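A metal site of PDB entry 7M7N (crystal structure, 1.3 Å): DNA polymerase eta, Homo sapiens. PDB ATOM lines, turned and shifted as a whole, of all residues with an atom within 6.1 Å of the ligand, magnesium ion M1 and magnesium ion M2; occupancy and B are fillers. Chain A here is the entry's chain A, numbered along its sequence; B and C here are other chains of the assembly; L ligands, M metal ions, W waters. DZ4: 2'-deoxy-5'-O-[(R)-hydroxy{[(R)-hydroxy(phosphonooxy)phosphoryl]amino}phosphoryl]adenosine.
N6 of AF2 8 of chain B lies within hydrogen-bond range of N6 of the ligand. The side-chain hydroxyl of Tyr 55 lies within hydrogen-bond range of an oxygen (O2G) of the ligand. O4 of DT 4 of chain C sits at hydrogen-bond distance from a nitrogen (N6) of the ligand, 3.0 Å away. The backbone NH (N) of Cys 19 is in hydrogen-bond range of an oxygen (O2G) of the ligand, 2.9 Å away. The guanidinium group (NH1) of Arg 64 lies within hydrogen-bond range of a nitrogen (N7) of the ligand. The guanidinium group of Arg 58 lies within salt-bridge range of an oxygen (O3G) of the ligand, 3.1 Å away. An oxygen (O2B) of the ligand is in hydrogen-bond range of the backbone NH (N) of Phe 20. O3' of the ligand is in hydrogen-bond range of N of Phe 21. O2G of the ligand is in salt-bridge range of NZ of Lys 234 (3.1 Å).
OG of Ser 116 lies close to N of Glu 119 (3.4 Å). NZ of Lys 227 lies within salt-bridge range of OE1 of Glu 119. O3' of AF2 8 of chain B lies close to the side-chain hydroxyl (OG) of Ser 116 (2.9 Å). The side-chain amino group of Lys 227 is in salt-bridge range of OP1 of AF2 8 of chain B (3.0 Å). OH of Tyr 55 lies within hydrogen-bond range of NH1 of Arg 58 (3.2 Å). O2 of DT 4 of chain C sits at hydrogen-bond distance from NE2 of Gln 41, 3.1 Å away. The guanidinium group (NE) of Arg 58 is in hydrogen-bond range of the backbone carbonyl oxygen (O) of Val 53 (2.9 Å). The side-chain amino group (NZ) of Lys 234 is in salt-bridge range of the side-chain carboxylate (OD1) of Asp 18 (2.9 Å).
Merely in contact with the ligand: Asp 18 (3.3 Å), Ile 51 (3.3 Å), DT 5 of chain C (3.6 Å), Ala 52 (3.6 Å) and Ile 117 (3.8 Å). Along chain A the residues within 4 Å of the ligand span positions 16 to 234. The nearest printed residue that does not touch the ligand is Glu 119 (4.3 Å).
OG of Ser 116 touches magnesium ion M1 (3.7 Å). Of the 25 residues printed, 5 come within 4 Å of magnesium ion M1. The nearest printed residue that does not touch magnesium ion M1 is Lys 227 (4.4 Å).
Lys 234 touches magnesium ion M2. Of the 25 residues printed, 4 come within 4 Å of magnesium ion M2. Along chain A the residues within 4 Å of magnesium ion M2 span positions 16 to 234. The nearest printed residue that does not touch magnesium ion M2 is Asp 18 (4.4 Å).
Magnesium ion M1 is bound by OD2 of Asp 16 (2.1 Å). The side-chain carboxylate (OD1) of Asp 118 binds magnesium ion M1. Water W3 is bound to magnesium ion M1 (2.1 Å). Magnesium ion M1 is bound by OE2 of Glu 119, at 2.1 Å. O3' of AF2 8 of chain B binds magnesium ion M1, 2.1 Å away. O1A of the ligand binds magnesium ion M1 (2.2 Å). Magnesium ion M1 has six donor atoms within binding distance.
Magnesium ion M2 is bound by OD2 of Asp 118 (2.0 Å), OD1 of Asp 16 (2.1 Å), O of Met 17 (2.1 Å), O1G of the ligand (2.2 Å), O1B of the ligand (2.2 Å) and O1A of the ligand (2.3 Å).
Water W3 lies within hydrogen-bond range of O2A of the ligand, NZ of Lys 227 and O5' of AF2 8 of chain B. Water W8 lies within hydrogen-bond range of an oxygen (O2B) of the ligand (2.6 Å), the backbone NH (N) of Val 53 (2.9 Å) and the guanidinium group (NH2) of Arg 58 (2.9 Å). Water W6 lies within hydrogen-bond range of O2A of the ligand, OP2 of AF2 8 of chain B and NH1 of Arg 64. Water W4 bridges N3 of AF2 8 of chain B (2.9 Å) and an oxygen (O4') of the ligand (3.1 Å). Water W1 lies within hydrogen-bond range of the backbone carbonyl oxygen of Ile 51 (3.0 Å) and a nitrogen (N3A) of the ligand (3.4 Å).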
ATOM      1  N   ASP A  16      -0.262  19.246 -13.412  1.00  0.00           N
ATOM      2  CA  ASP A  16      -0.718  18.868 -14.746  1.00  0.00           C
ATOM      3  C   ASP A  16       0.443  18.310 -15.549  1.00  0.00           C
ATOM      4  O   ASP A  16       1.491  18.960 -15.693  1.00  0.00           O
ATOM      5  CB  ASP A  16      -1.318  20.060 -15.495  1.00  0.00           C
ATOM      6  CG  ASP A  16      -1.908  19.666 -16.808  1.00  0.00           C
ATOM      7  OD1 ASP A  16      -1.115  19.431 -17.740  1.00  0.00           O
ATOM      8  OD2 ASP A  16      -3.144  19.581 -16.896  1.00  0.00           O
ATOM      9  N   MET A  17       0.254  17.097 -16.069  1.00  0.00           N
ATOM     10  CA  MET A  17       1.343  16.428 -16.773  1.00  0.00           C
ATOM     11  C   MET A  17       1.689  17.133 -18.071  1.00  0.00           C
ATOM     12  O   MET A  17       0.828  17.680 -18.773  1.00  0.00           O
ATOM     13  CB  MET A  17       0.946  14.972 -17.074  1.00  0.00           C
ATOM     14  CG  MET A  17       0.501  14.171 -15.846  1.00  0.00           C
ATOM     15  SD  MET A  17       1.685  14.168 -14.488  1.00  0.00           S
ATOM     16  CE  MET A  17       3.040  13.345 -15.261  1.00  0.00           C
ATOM     17  N   ASP A  18       2.981  17.161 -18.399  1.00  0.00           N
ATOM     18  CA  ASP A  18       3.409  17.770 -19.651  1.00  0.00           C
ATOM     19  C   ASP A  18       3.144  16.817 -20.811  1.00  0.00           C
ATOM     20  O   ASP A  18       3.443  15.608 -20.706  1.00  0.00           O
ATOM     21  CB  ASP A  18       4.882  18.135 -19.603  1.00  0.00           C
ATOM     22  CG  ASP A  18       5.204  19.175 -18.539  1.00  0.00           C
ATOM     23  OD1 ASP A  18       4.338  19.998 -18.187  1.00  0.00           O
ATOM     24  OD2 ASP A  18       6.350  19.166 -18.052  1.00  0.00           O
ATOM     25  N   CYS A  19       2.559  17.338 -21.889  1.00  0.00           N
ATOM     26  CA  CYS A  19       2.208  16.562 -23.092  1.00  0.00           C
ATOM     27  C   CYS A  19       1.940  15.093 -22.779  1.00  0.00           C
ATOM     28  O   CYS A  19       2.634  14.199 -23.281  1.00  0.00           O
ATOM     29  CB  CYS A  19       3.238  16.762 -24.214  1.00  0.00           C
ATOM     30  SG  CYS A  19       4.969  16.407 -23.805  1.00  0.00           S
ATOM     31  N   PHE A  20       0.923  14.837 -21.962  1.00  0.00           N
ATOM     32  CA  PHE A  20       0.841  13.588 -21.211  1.00  0.00           C
ATOM     33  C   PHE A  20       0.881  12.349 -22.102  1.00  0.00           C
ATOM     34  O   PHE A  20       1.719  11.453 -21.885  1.00  0.00           O
ATOM     35  CB  PHE A  20      -0.383  13.586 -20.307  1.00  0.00           C
ATOM     36  CG  PHE A  20      -0.503  12.360 -19.453  1.00  0.00           C
ATOM     37  CD1 PHE A  20       0.582  11.900 -18.737  1.00  0.00           C
ATOM     38  CD2 PHE A  20      -1.713  11.694 -19.363  1.00  0.00           C
ATOM     39  CE1 PHE A  20       0.477  10.769 -17.939  1.00  0.00           C
ATOM     40  CE2 PHE A  20      -1.839  10.569 -18.571  1.00  0.00           C
ATOM     41  CZ  PHE A  20      -0.741  10.110 -17.848  1.00  0.00           C
ATOM     42  N   PHE A  21      -0.034  12.228 -23.083  1.00  0.00           N
ATOM     43  CA  PHE A  21      -0.050  10.968 -23.832  1.00  0.00           C
ATOM     44  C   PHE A  21       1.249  10.770 -24.597  1.00  0.00           C
ATOM     45  O   PHE A  21       1.707   9.621 -24.783  1.00  0.00           O
ATOM     46  CB  PHE A  21      -1.216  10.892 -24.825  1.00  0.00           C
ATOM     47  CG  PHE A  21      -2.598  10.782 -24.206  1.00  0.00           C
ATOM     48  CD1 PHE A  21      -2.834  10.964 -22.852  1.00  0.00           C
ATOM     49  CD2 PHE A  21      -3.678  10.518 -25.033  1.00  0.00           C
ATOM     50  CE1 PHE A  21      -4.143  10.878 -22.327  1.00  0.00           C
ATOM     51  CE2 PHE A  21      -4.969  10.408 -24.530  1.00  0.00           C
ATOM     52  CZ  PHE A  21      -5.202  10.613 -23.186  1.00  0.00           C
ATOM     53  N   VAL A  22       1.879  11.861 -25.042  1.00  0.00           N
ATOM     54  CA  VAL A  22       3.186  11.750 -25.691  1.00  0.00           C
ATOM     55  C   VAL A  22       4.208  11.148 -24.740  1.00  0.00           C
ATOM     56  O   VAL A  22       4.973  10.254 -25.106  1.00  0.00           O
ATOM     57  CB  VAL A  22       3.633  13.114 -26.245  1.00  0.00           C
ATOM     58  CG1 VAL A  22       5.099  13.063 -26.630  1.00  0.00           C
ATOM     59  CG2 VAL A  22       2.755  13.508 -27.421  1.00  0.00           C
ATOM     60  N   GLN A  41      -5.134   9.502 -33.328  1.00  0.00           N
ATOM     61  CA  GLN A  41      -6.208   8.519 -33.334  1.00  0.00           C
ATOM     62  C   GLN A  41      -6.613   8.275 -34.774  1.00  0.00           C
ATOM     63  O   GLN A  41      -6.905   9.224 -35.507  1.00  0.00           O
ATOM     64  CB  GLN A  41      -7.420   9.008 -32.537  1.00  0.00           C
ATOM     65  CG  GLN A  41      -7.234   8.874 -31.054  1.00  0.00           C
ATOM     66  CD  GLN A  41      -8.428   9.334 -30.243  1.00  0.00           C
ATOM     67  OE1 GLN A  41      -8.772   8.711 -29.248  1.00  0.00           O
ATOM     68  NE2 GLN A  41      -9.054  10.440 -30.650  1.00  0.00           N
ATOM     69  N   ILE A  51      -4.073  14.282 -30.854  1.00  0.00           N
ATOM     70  CA  ILE A  51      -4.615  14.608 -29.533  1.00  0.00           C
ATOM     71  C   ILE A  51      -3.560  15.026 -28.519  1.00  0.00           C
ATOM     72  O   ILE A  51      -3.944  15.473 -27.421  1.00  0.00           O
ATOM     73  CB  ILE A  51      -5.529  13.488 -28.973  1.00  0.00           C
ATOM     74  CG1 ILE A  51      -4.783  12.160 -28.822  1.00  0.00           C
ATOM     75  CG2 ILE A  51      -6.807  13.363 -29.816  1.00  0.00           C
ATOM     76  CD1 ILE A  51      -5.613  11.076 -28.137  1.00  0.00           C
ATOM     77  N   ALA A  52      -2.266  14.916 -28.826  1.00  0.00           N
ATOM     78  CA  ALA A  52      -1.221  15.381 -27.913  1.00  0.00           C
ATOM     79  C   ALA A  52       0.048  15.608 -28.719  1.00  0.00           C
ATOM     80  O   ALA A  52       0.307  14.908 -29.698  1.00  0.00           O
ATOM     81  CB  ALA A  52      -0.960  14.354 -26.796  1.00  0.00           C
ATOM     82  N   VAL A  53       0.849  16.602 -28.293  1.00  0.00           N
ATOM     83  CA  VAL A  53       1.965  17.114 -29.084  1.00  0.00           C
ATOM     84  C   VAL A  53       3.138  17.412 -28.154  1.00  0.00           C
ATOM     85  O   VAL A  53       2.986  18.141 -27.173  1.00  0.00           O
ATOM     86  CB  VAL A  53       1.586  18.409 -29.847  1.00  0.00           C
ATOM     87  CG1 VAL A  53       2.719  18.851 -30.743  1.00  0.00           C
ATOM     88  CG2 VAL A  53       0.284  18.229 -30.635  1.00  0.00           C
ATOM     89  N   TYR A  55       6.644  19.147 -26.903  1.00  0.00           N
ATOM     90  CA  TYR A  55       7.056  20.554 -26.978  1.00  0.00           C
ATOM     91  C   TYR A  55       7.968  20.819 -28.169  1.00  0.00           C
ATOM     92  O   TYR A  55       7.867  21.889 -28.814  1.00  0.00           O
ATOM     93  CB  TYR A  55       7.617  21.008 -25.623  1.00  0.00           C
ATOM     94  CG  TYR A  55       6.509  21.281 -24.646  1.00  0.00           C
ATOM     95  CD1 TYR A  55       5.877  20.249 -23.956  1.00  0.00           C
ATOM     96  CD2 TYR A  55       6.027  22.569 -24.466  1.00  0.00           C
ATOM     97  CE1 TYR A  55       4.830  20.498 -23.099  1.00  0.00           C
ATOM     98  CE2 TYR A  55       4.993  22.835 -23.604  1.00  0.00           C
ATOM     99  CZ  TYR A  55       4.380  21.797 -22.922  1.00  0.00           C
ATOM    100  OH  TYR A  55       3.337  22.068 -22.074  1.00  0.00           O
ATOM    101  N   ARG A  58       5.607  21.302 -30.940  1.00  0.00           N
ATOM    102  CA  ARG A  58       4.901  22.575 -30.828  1.00  0.00           C
ATOM    103  C   ARG A  58       5.733  23.718 -31.381  1.00  0.00           C
ATOM    104  O   ARG A  58       5.176  24.691 -31.903  1.00  0.00           O
ATOM    105  CB  ARG A  58       4.506  22.872 -29.386  1.00  0.00           C
ATOM    106  CG  ARG A  58       3.604  21.831 -28.753  1.00  0.00           C
ATOM    107  CD  ARG A  58       3.187  22.203 -27.334  1.00  0.00           C
ATOM    108  NE  ARG A  58       2.642  21.019 -26.658  1.00  0.00           N
ATOM    109  CZ  ARG A  58       1.986  21.030 -25.502  1.00  0.00           C
ATOM    110  NH1 ARG A  58       1.757  22.163 -24.855  1.00  0.00           N
ATOM    111  NH2 ARG A  58       1.552  19.878 -24.989  1.00  0.00           N
ATOM    112  N   ARG A  64      -2.859  20.227 -31.263  1.00  0.00           N
ATOM    113  CA  ARG A  64      -3.990  19.322 -31.111  1.00  0.00           C
ATOM    114  C   ARG A  64      -5.055  19.683 -32.145  1.00  0.00           C
ATOM    115  O   ARG A  64      -5.182  20.835 -32.563  1.00  0.00           O
ATOM    116  CB  ARG A  64      -4.566  19.490 -29.708  1.00  0.00           C
ATOM    117  CG  ARG A  64      -5.740  18.609 -29.339  1.00  0.00           C
ATOM    118  CD  ARG A  64      -6.104  18.809 -27.874  1.00  0.00           C
ATOM    119  NE  ARG A  64      -6.986  19.949 -27.658  1.00  0.00           N
ATOM    120  CZ  ARG A  64      -7.136  20.561 -26.487  1.00  0.00           C
ATOM    121  NH1 ARG A  64      -6.446  20.155 -25.426  1.00  0.00           N
ATOM    122  NH2 ARG A  64      -7.968  21.591 -26.377  1.00  0.00           N
ATOM    123  N   SER A 116      -8.694  15.814 -14.331  1.00  0.00           N
ATOM    124  CA  SER A 116      -8.725  15.257 -15.672  1.00  0.00           C
ATOM    125  C   SER A 116      -7.813  14.053 -15.673  1.00  0.00           C
ATOM    126  O   SER A 116      -7.150  13.753 -14.680  1.00  0.00           O
ATOM    127  CB  SER A 116      -8.279  16.268 -16.740  1.00  0.00           C
ATOM    128  OG  SER A 116      -6.864  16.282 -16.910  1.00  0.00           O
ATOM    129  N   ILE A 117      -7.737  13.389 -16.835  1.00  0.00           N
ATOM    130  CA  ILE A 117      -6.838  12.249 -16.967  1.00  0.00           C
ATOM    131  C   ILE A 117      -5.405  12.598 -16.586  1.00  0.00           C
ATOM    132  O   ILE A 117      -4.631  11.716 -16.192  1.00  0.00           O
ATOM    133  CB  ILE A 117      -6.938  11.635 -18.376  1.00  0.00           C
ATOM    134  CG1 ILE A 117      -6.356  10.213 -18.374  1.00  0.00           C
ATOM    135  CG2 ILE A 117      -6.250  12.552 -19.393  1.00  0.00           C
ATOM    136  CD1 ILE A 117      -6.684   9.423 -19.629  1.00  0.00           C
ATOM    137  N   ASP A 118      -5.001  13.875 -16.689  1.00  0.00           N
ATOM    138  CA  ASP A 118      -3.598  14.212 -16.433  1.00  0.00           C
ATOM    139  C   ASP A 118      -3.428  15.280 -15.376  1.00  0.00           C
ATOM    140  O   ASP A 118      -2.350  15.885 -15.307  1.00  0.00           O
ATOM    141  CB  ASP A 118      -2.854  14.576 -17.719  1.00  0.00           C
ATOM    142  CG  ASP A 118      -2.864  16.069 -18.018  1.00  0.00           C
ATOM    143  OD1 ASP A 118      -3.918  16.729 -17.809  1.00  0.00           O
ATOM    144  OD2 ASP A 118      -1.803  16.559 -18.461  1.00  0.00           O
ATOM    145  N   GLU A 119      -4.450  15.550 -14.558  1.00  0.00           N
ATOM    146  CA  GLU A 119      -4.212  16.620 -13.587  1.00  0.00           C
ATOM    147  C   GLU A 119      -5.066  16.432 -12.356  1.00  0.00           C
ATOM    148  O   GLU A 119      -6.185  15.892 -12.424  1.00  0.00           O
ATOM    149  CB  GLU A 119      -4.443  18.017 -14.164  1.00  0.00           C
ATOM    150  CG  GLU A 119      -5.883  18.400 -14.377  1.00  0.00           C
ATOM    151  CD  GLU A 119      -6.012  19.325 -15.559  1.00  0.00           C
ATOM    152  OE1 GLU A 119      -6.251  20.539 -15.365  1.00  0.00           O
ATOM    153  OE2 GLU A 119      -5.841  18.842 -16.697  1.00  0.00           O
ATOM    154  N   LYS A 227      -4.520  26.613 -11.179  1.00  0.00           N
ATOM    155  CA  LYS A 227      -4.588  26.180 -12.565  1.00  0.00           C
ATOM    156  C   LYS A 227      -3.948  27.211 -13.498  1.00  0.00           C
ATOM    157  O   LYS A 227      -3.151  26.857 -14.381  1.00  0.00           O
ATOM    158  CB  LYS A 227      -6.047  25.917 -12.962  1.00  0.00           C
ATOM    159  CG  LYS A 227      -6.257  25.589 -14.453  1.00  0.00           C
ATOM    160  CD  LYS A 227      -5.575  24.276 -14.888  1.00  0.00           C
ATOM    161  CE  LYS A 227      -6.015  23.929 -16.297  1.00  0.00           C
ATOM    162  NZ  LYS A 227      -5.361  22.707 -16.848  1.00  0.00           N
ATOM    163  N   LYS A 234       4.946  26.160 -17.997  1.00  0.00           N
ATOM    164  CA  LYS A 234       5.090  24.854 -18.632  1.00  0.00           C
ATOM    165  C   LYS A 234       6.123  24.937 -19.755  1.00  0.00           C
ATOM    166  O   LYS A 234       6.179  25.940 -20.469  1.00  0.00           O
ATOM    167  CB  LYS A 234       3.759  24.445 -19.255  1.00  0.00           C
ATOM    168  CG  LYS A 234       3.012  23.449 -18.434  1.00  0.00           C
ATOM    169  CD  LYS A 234       1.712  23.034 -19.074  1.00  0.00           C
ATOM    170  CE  LYS A 234       1.007  22.037 -18.171  1.00  0.00           C
ATOM    171  NZ  LYS A 234       1.546  20.652 -18.316  1.00  0.00           N
ATOM    172  N   PRO A 235       6.910  23.872 -19.986  1.00  0.00           N
ATOM    173  CA  PRO A 235       6.856  22.580 -19.277  1.00  0.00           C
ATOM    174  C   PRO A 235       7.909  22.454 -18.177  1.00  0.00           C
ATOM    175  O   PRO A 235       8.846  23.255 -18.097  1.00  0.00           O
ATOM    176  CB  PRO A 235       7.182  21.590 -20.390  1.00  0.00           C
ATOM    177  CG  PRO A 235       8.165  22.335 -21.244  1.00  0.00           C
ATOM    178  CD  PRO A 235       7.780  23.802 -21.169  1.00  0.00           C
ATOM    179  P    DA B   7     -13.422  26.728 -20.462  1.00  0.00           P
ATOM    180  OP1  DA B   7     -12.839  27.714 -19.529  1.00  0.00           O
ATOM    181  OP2  DA B   7     -13.523  27.045 -21.885  1.00  0.00           O
ATOM    182  O5'  DA B   7     -12.625  25.343 -20.406  1.00  0.00           O
ATOM    183  C5'  DA B   7     -12.476  24.667 -19.211  1.00  0.00           C
ATOM    184  C4'  DA B   7     -11.966  23.271 -19.467  1.00  0.00           C
ATOM    185  O4'  DA B   7     -12.980  22.484 -20.138  1.00  0.00           O
ATOM    186  C3'  DA B   7     -10.717  23.187 -20.368  1.00  0.00           C
ATOM    187  O3'  DA B   7      -9.667  22.673 -19.588  1.00  0.00           O
ATOM    188  C2'  DA B   7     -11.122  22.226 -21.477  1.00  0.00           C
ATOM    189  C1'  DA B   7     -12.331  21.514 -20.865  1.00  0.00           C
ATOM    190  N9   DA B   7     -13.246  20.981 -21.859  1.00  0.00           N
ATOM    191  C8   DA B   7     -13.908  21.675 -22.824  1.00  0.00           C
ATOM    192  N7   DA B   7     -14.634  20.923 -23.606  1.00  0.00           N
ATOM    193  C5   DA B   7     -14.415  19.636 -23.125  1.00  0.00           C
ATOM    194  C6   DA B   7     -14.896  18.383 -23.528  1.00  0.00           C
ATOM    195  N6   DA B   7     -15.731  18.207 -24.564  1.00  0.00           N
ATOM    196  N1   DA B   7     -14.471  17.298 -22.845  1.00  0.00           N
ATOM    197  C2   DA B   7     -13.628  17.469 -21.809  1.00  0.00           C
ATOM    198  N3   DA B   7     -13.116  18.604 -21.332  1.00  0.00           N
ATOM    199  C4   DA B   7     -13.553  19.658 -22.055  1.00  0.00           C
ATOM    200  F   AF2 B   8      -7.693  16.011 -20.020  1.00  0.00           F
ATOM    201  P   AF2 B   8      -8.165  22.581 -20.102  1.00  0.00           P
ATOM    202  N1  AF2 B   8     -11.604  15.725 -25.073  1.00  0.00           N
ATOM    203  C2  AF2 B   8     -11.024  15.116 -24.032  1.00  0.00           C
ATOM    204  N3  AF2 B   8     -10.392  15.645 -22.995  1.00  0.00           N
ATOM    205  C4  AF2 B   8     -10.384  16.988 -23.082  1.00  0.00           C
ATOM    206  C5  AF2 B   8     -10.919  17.761 -24.093  1.00  0.00           C
ATOM    207  C6  AF2 B   8     -11.577  17.075 -25.134  1.00  0.00           C
ATOM    208  N6  AF2 B   8     -12.149  17.679 -26.175  1.00  0.00           N
ATOM    209  N7  AF2 B   8     -10.710  19.115 -23.852  1.00  0.00           N
ATOM    210  C8  AF2 B   8     -10.051  19.123 -22.725  1.00  0.00           C
ATOM    211  N9  AF2 B   8      -9.776  17.878 -22.217  1.00  0.00           N
ATOM    212  C1' AF2 B   8      -9.209  17.537 -20.919  1.00  0.00           C
ATOM    213  OP2 AF2 B   8      -8.026  23.008 -21.514  1.00  0.00           O
ATOM    214  C2' AF2 B   8      -7.742  17.118 -20.836  1.00  0.00           C
ATOM    215  OP1 AF2 B   8      -7.324  23.214 -19.070  1.00  0.00           O
ATOM    216  C3' AF2 B   8      -7.110  18.274 -20.073  1.00  0.00           C
ATOM    217  O3' AF2 B   8      -6.058  17.809 -19.246  1.00  0.00           O
ATOM    218  C4' AF2 B   8      -8.249  18.807 -19.215  1.00  0.00           C
ATOM    219  O4' AF2 B   8      -9.409  18.641 -20.061  1.00  0.00           O
ATOM    220  C5' AF2 B   8      -8.120  20.260 -18.850  1.00  0.00           C
ATOM    221  O5' AF2 B   8      -7.892  21.016 -20.061  1.00  0.00           O
ATOM    222  P    DT C   4     -14.333  14.351 -35.530  1.00  0.00           P
ATOM    223  OP1  DT C   4     -15.062  13.490 -36.490  1.00  0.00           O
ATOM    224  OP2  DT C   4     -15.024  15.377 -34.730  1.00  0.00           O
ATOM    225  O5'  DT C   4     -13.623  13.371 -34.483  1.00  0.00           O
ATOM    226  C5'  DT C   4     -12.807  12.317 -34.939  1.00  0.00           C
ATOM    227  C4'  DT C   4     -12.400  11.437 -33.773  1.00  0.00           C
ATOM    228  O4'  DT C   4     -11.655  12.217 -32.810  1.00  0.00           O
ATOM    229  C3'  DT C   4     -13.556  10.802 -33.007  1.00  0.00           C
ATOM    230  O3'  DT C   4     -13.148   9.543 -32.555  1.00  0.00           O
ATOM    231  C2'  DT C   4     -13.763  11.784 -31.849  1.00  0.00           C
ATOM    232  C1'  DT C   4     -12.335  12.220 -31.565  1.00  0.00           C
ATOM    233  N1   DT C   4     -12.178  13.571 -30.963  1.00  0.00           N
ATOM    234  C2   DT C   4     -11.305  13.696 -29.907  1.00  0.00           C
ATOM    235  O2   DT C   4     -10.720  12.750 -29.433  1.00  0.00           O
ATOM    236  N3   DT C   4     -11.172  14.954 -29.419  1.00  0.00           N
ATOM    237  C4   DT C   4     -11.783  16.103 -29.880  1.00  0.00           C
ATOM    238  O4   DT C   4     -11.579  17.201 -29.355  1.00  0.00           O
ATOM    239  C5   DT C   4     -12.681  15.917 -31.001  1.00  0.00           C
ATOM    240  C7   DT C   4     -13.420  17.088 -31.592  1.00  0.00           C
ATOM    241  C6   DT C   4     -12.818  14.670 -31.497  1.00  0.00           C
ATOM    242  P    DT C   5     -14.169   8.579 -31.777  1.00  0.00           P
ATOM    243  OP1  DT C   5     -13.861   7.213 -32.242  1.00  0.00           O
ATOM    244  OP2  DT C   5     -15.563   9.084 -31.873  1.00  0.00           O
ATOM    245  O5'  DT C   5     -13.710   8.736 -30.246  1.00  0.00           O
ATOM    246  C5'  DT C   5     -12.438   8.272 -29.826  1.00  0.00           C
ATOM    247  C4'  DT C   5     -12.259   8.508 -28.348  1.00  0.00           C
ATOM    248  O4'  DT C   5     -12.143   9.937 -28.110  1.00  0.00           O
ATOM    249  C3'  DT C   5     -13.431   8.047 -27.469  1.00  0.00           C
ATOM    250  O3'  DT C   5     -12.911   7.493 -26.261  1.00  0.00           O
ATOM    251  C2'  DT C   5     -14.193   9.350 -27.217  1.00  0.00           C
ATOM    252  C1'  DT C   5     -13.023  10.299 -27.076  1.00  0.00           C
ATOM    253  N1   DT C   5     -13.346  11.737 -27.227  1.00  0.00           N
ATOM    254  C2   DT C   5     -12.628  12.638 -26.488  1.00  0.00           C
ATOM    255  O2   DT C   5     -11.757  12.303 -25.713  1.00  0.00           O
ATOM    256  N3   DT C   5     -12.972  13.945 -26.686  1.00  0.00           N
ATOM    257  C4   DT C   5     -13.933  14.438 -27.546  1.00  0.00           C
ATOM    258  O4   DT C   5     -14.162  15.641 -27.650  1.00  0.00           O
ATOM    259  C5   DT C   5     -14.646  13.443 -28.308  1.00  0.00           C
ATOM    260  C7   DT C   5     -15.720  13.855 -29.272  1.00  0.00           C
ATOM    261  C6   DT C   5     -14.319  12.146 -28.123  1.00  0.00           C
HETATM  262  N1  DZ4 L   1      -9.370  15.215 -27.328  1.00  0.00           N
HETATM  263  C2  DZ4 L   1      -8.853  14.085 -26.830  1.00  0.00           C
HETATM  264  N3  DZ4 L   1      -7.897  13.926 -25.910  1.00  0.00           N
HETATM  265  C4  DZ4 L   1      -7.471  15.117 -25.470  1.00  0.00           C
HETATM  266  C5  DZ4 L   1      -7.902  16.357 -25.868  1.00  0.00           C
HETATM  267  C6  DZ4 L   1      -8.903  16.391 -26.856  1.00  0.00           C
HETATM  268  N6  DZ4 L   1      -9.391  17.540 -27.315  1.00  0.00           N
HETATM  269  N7  DZ4 L   1      -7.218  17.353 -25.181  1.00  0.00           N
HETATM  270  C8  DZ4 L   1      -6.398  16.706 -24.399  1.00  0.00           C
HETATM  271  N9  DZ4 L   1      -6.505  15.347 -24.521  1.00  0.00           N
HETATM  272  PA  DZ4 L   1      -3.765  18.532 -21.474  1.00  0.00           P
HETATM  273  PB  DZ4 L   1      -1.124  17.865 -22.567  1.00  0.00           P
HETATM  274  PG  DZ4 L   1       0.326  20.236 -21.670  1.00  0.00           P
HETATM  275  C1' DZ4 L   1      -5.767  14.302 -23.830  1.00  0.00           C
HETATM  276  O1A DZ4 L   1      -3.294  18.565 -20.101  1.00  0.00           O
HETATM  277  O1B DZ4 L   1      -0.851  17.168 -21.319  1.00  0.00           O
HETATM  278  O1G DZ4 L   1      -0.544  20.012 -20.471  1.00  0.00           O
HETATM  279  C2' DZ4 L   1      -4.365  14.109 -24.393  1.00  0.00           C
HETATM  280  O2A DZ4 L   1      -4.875  19.597 -21.679  1.00  0.00           O
HETATM  281  O2B DZ4 L   1      -0.923  16.915 -23.783  1.00  0.00           O
HETATM  282  O2G DZ4 L   1       1.781  20.038 -21.362  1.00  0.00           O
HETATM  283  C3' DZ4 L   1      -3.490  14.917 -23.445  1.00  0.00           C
HETATM  284  O3' DZ4 L   1      -2.167  14.400 -23.362  1.00  0.00           O
HETATM  285  N3A DZ4 L   1      -2.574  18.628 -22.585  1.00  0.00           N
HETATM  286  O3B DZ4 L   1      -0.063  19.065 -22.699  1.00  0.00           O
HETATM  287  O3G DZ4 L   1       0.045  21.541 -22.359  1.00  0.00           O
HETATM  288  C4' DZ4 L   1      -4.224  14.751 -22.121  1.00  0.00           C
HETATM  289  O4' DZ4 L   1      -5.619  14.676 -22.463  1.00  0.00           O
HETATM  290  C5' DZ4 L   1      -4.023  15.890 -21.156  1.00  0.00           C
HETATM  291  O5' DZ4 L   1      -4.496  17.124 -21.757  1.00  0.00           O
HETATM  292 MG    MG M   1      -4.402  18.688 -18.248  1.00  0.00          MG
HETATM  293 MG    MG M   2      -1.128  18.225 -19.418  1.00  0.00          MG
HETATM  294  O   HOH W   1      -3.467  17.927 -25.737  1.00  0.00           O
HETATM  295  O   HOH W   2      -2.073  21.339 -24.093  1.00  0.00           O
HETATM  296  O   HOH W   3      -4.853  20.603 -18.988  1.00  0.00           O
HETATM  297  O   HOH W   4      -8.523  13.795 -21.794  1.00  0.00           O
HETATM  298  O   HOH W   5      -8.180  11.212 -24.994  1.00  0.00           O
HETATM  299  O   HOH W   6      -5.686  21.934 -22.760  1.00  0.00           O
HETATM  300  O   HOH W   7      -2.373  21.772 -19.486  1.00  0.00           O
HETATM  301  O   HOH W   8      -0.404  18.008 -26.131  1.00  0.00           O
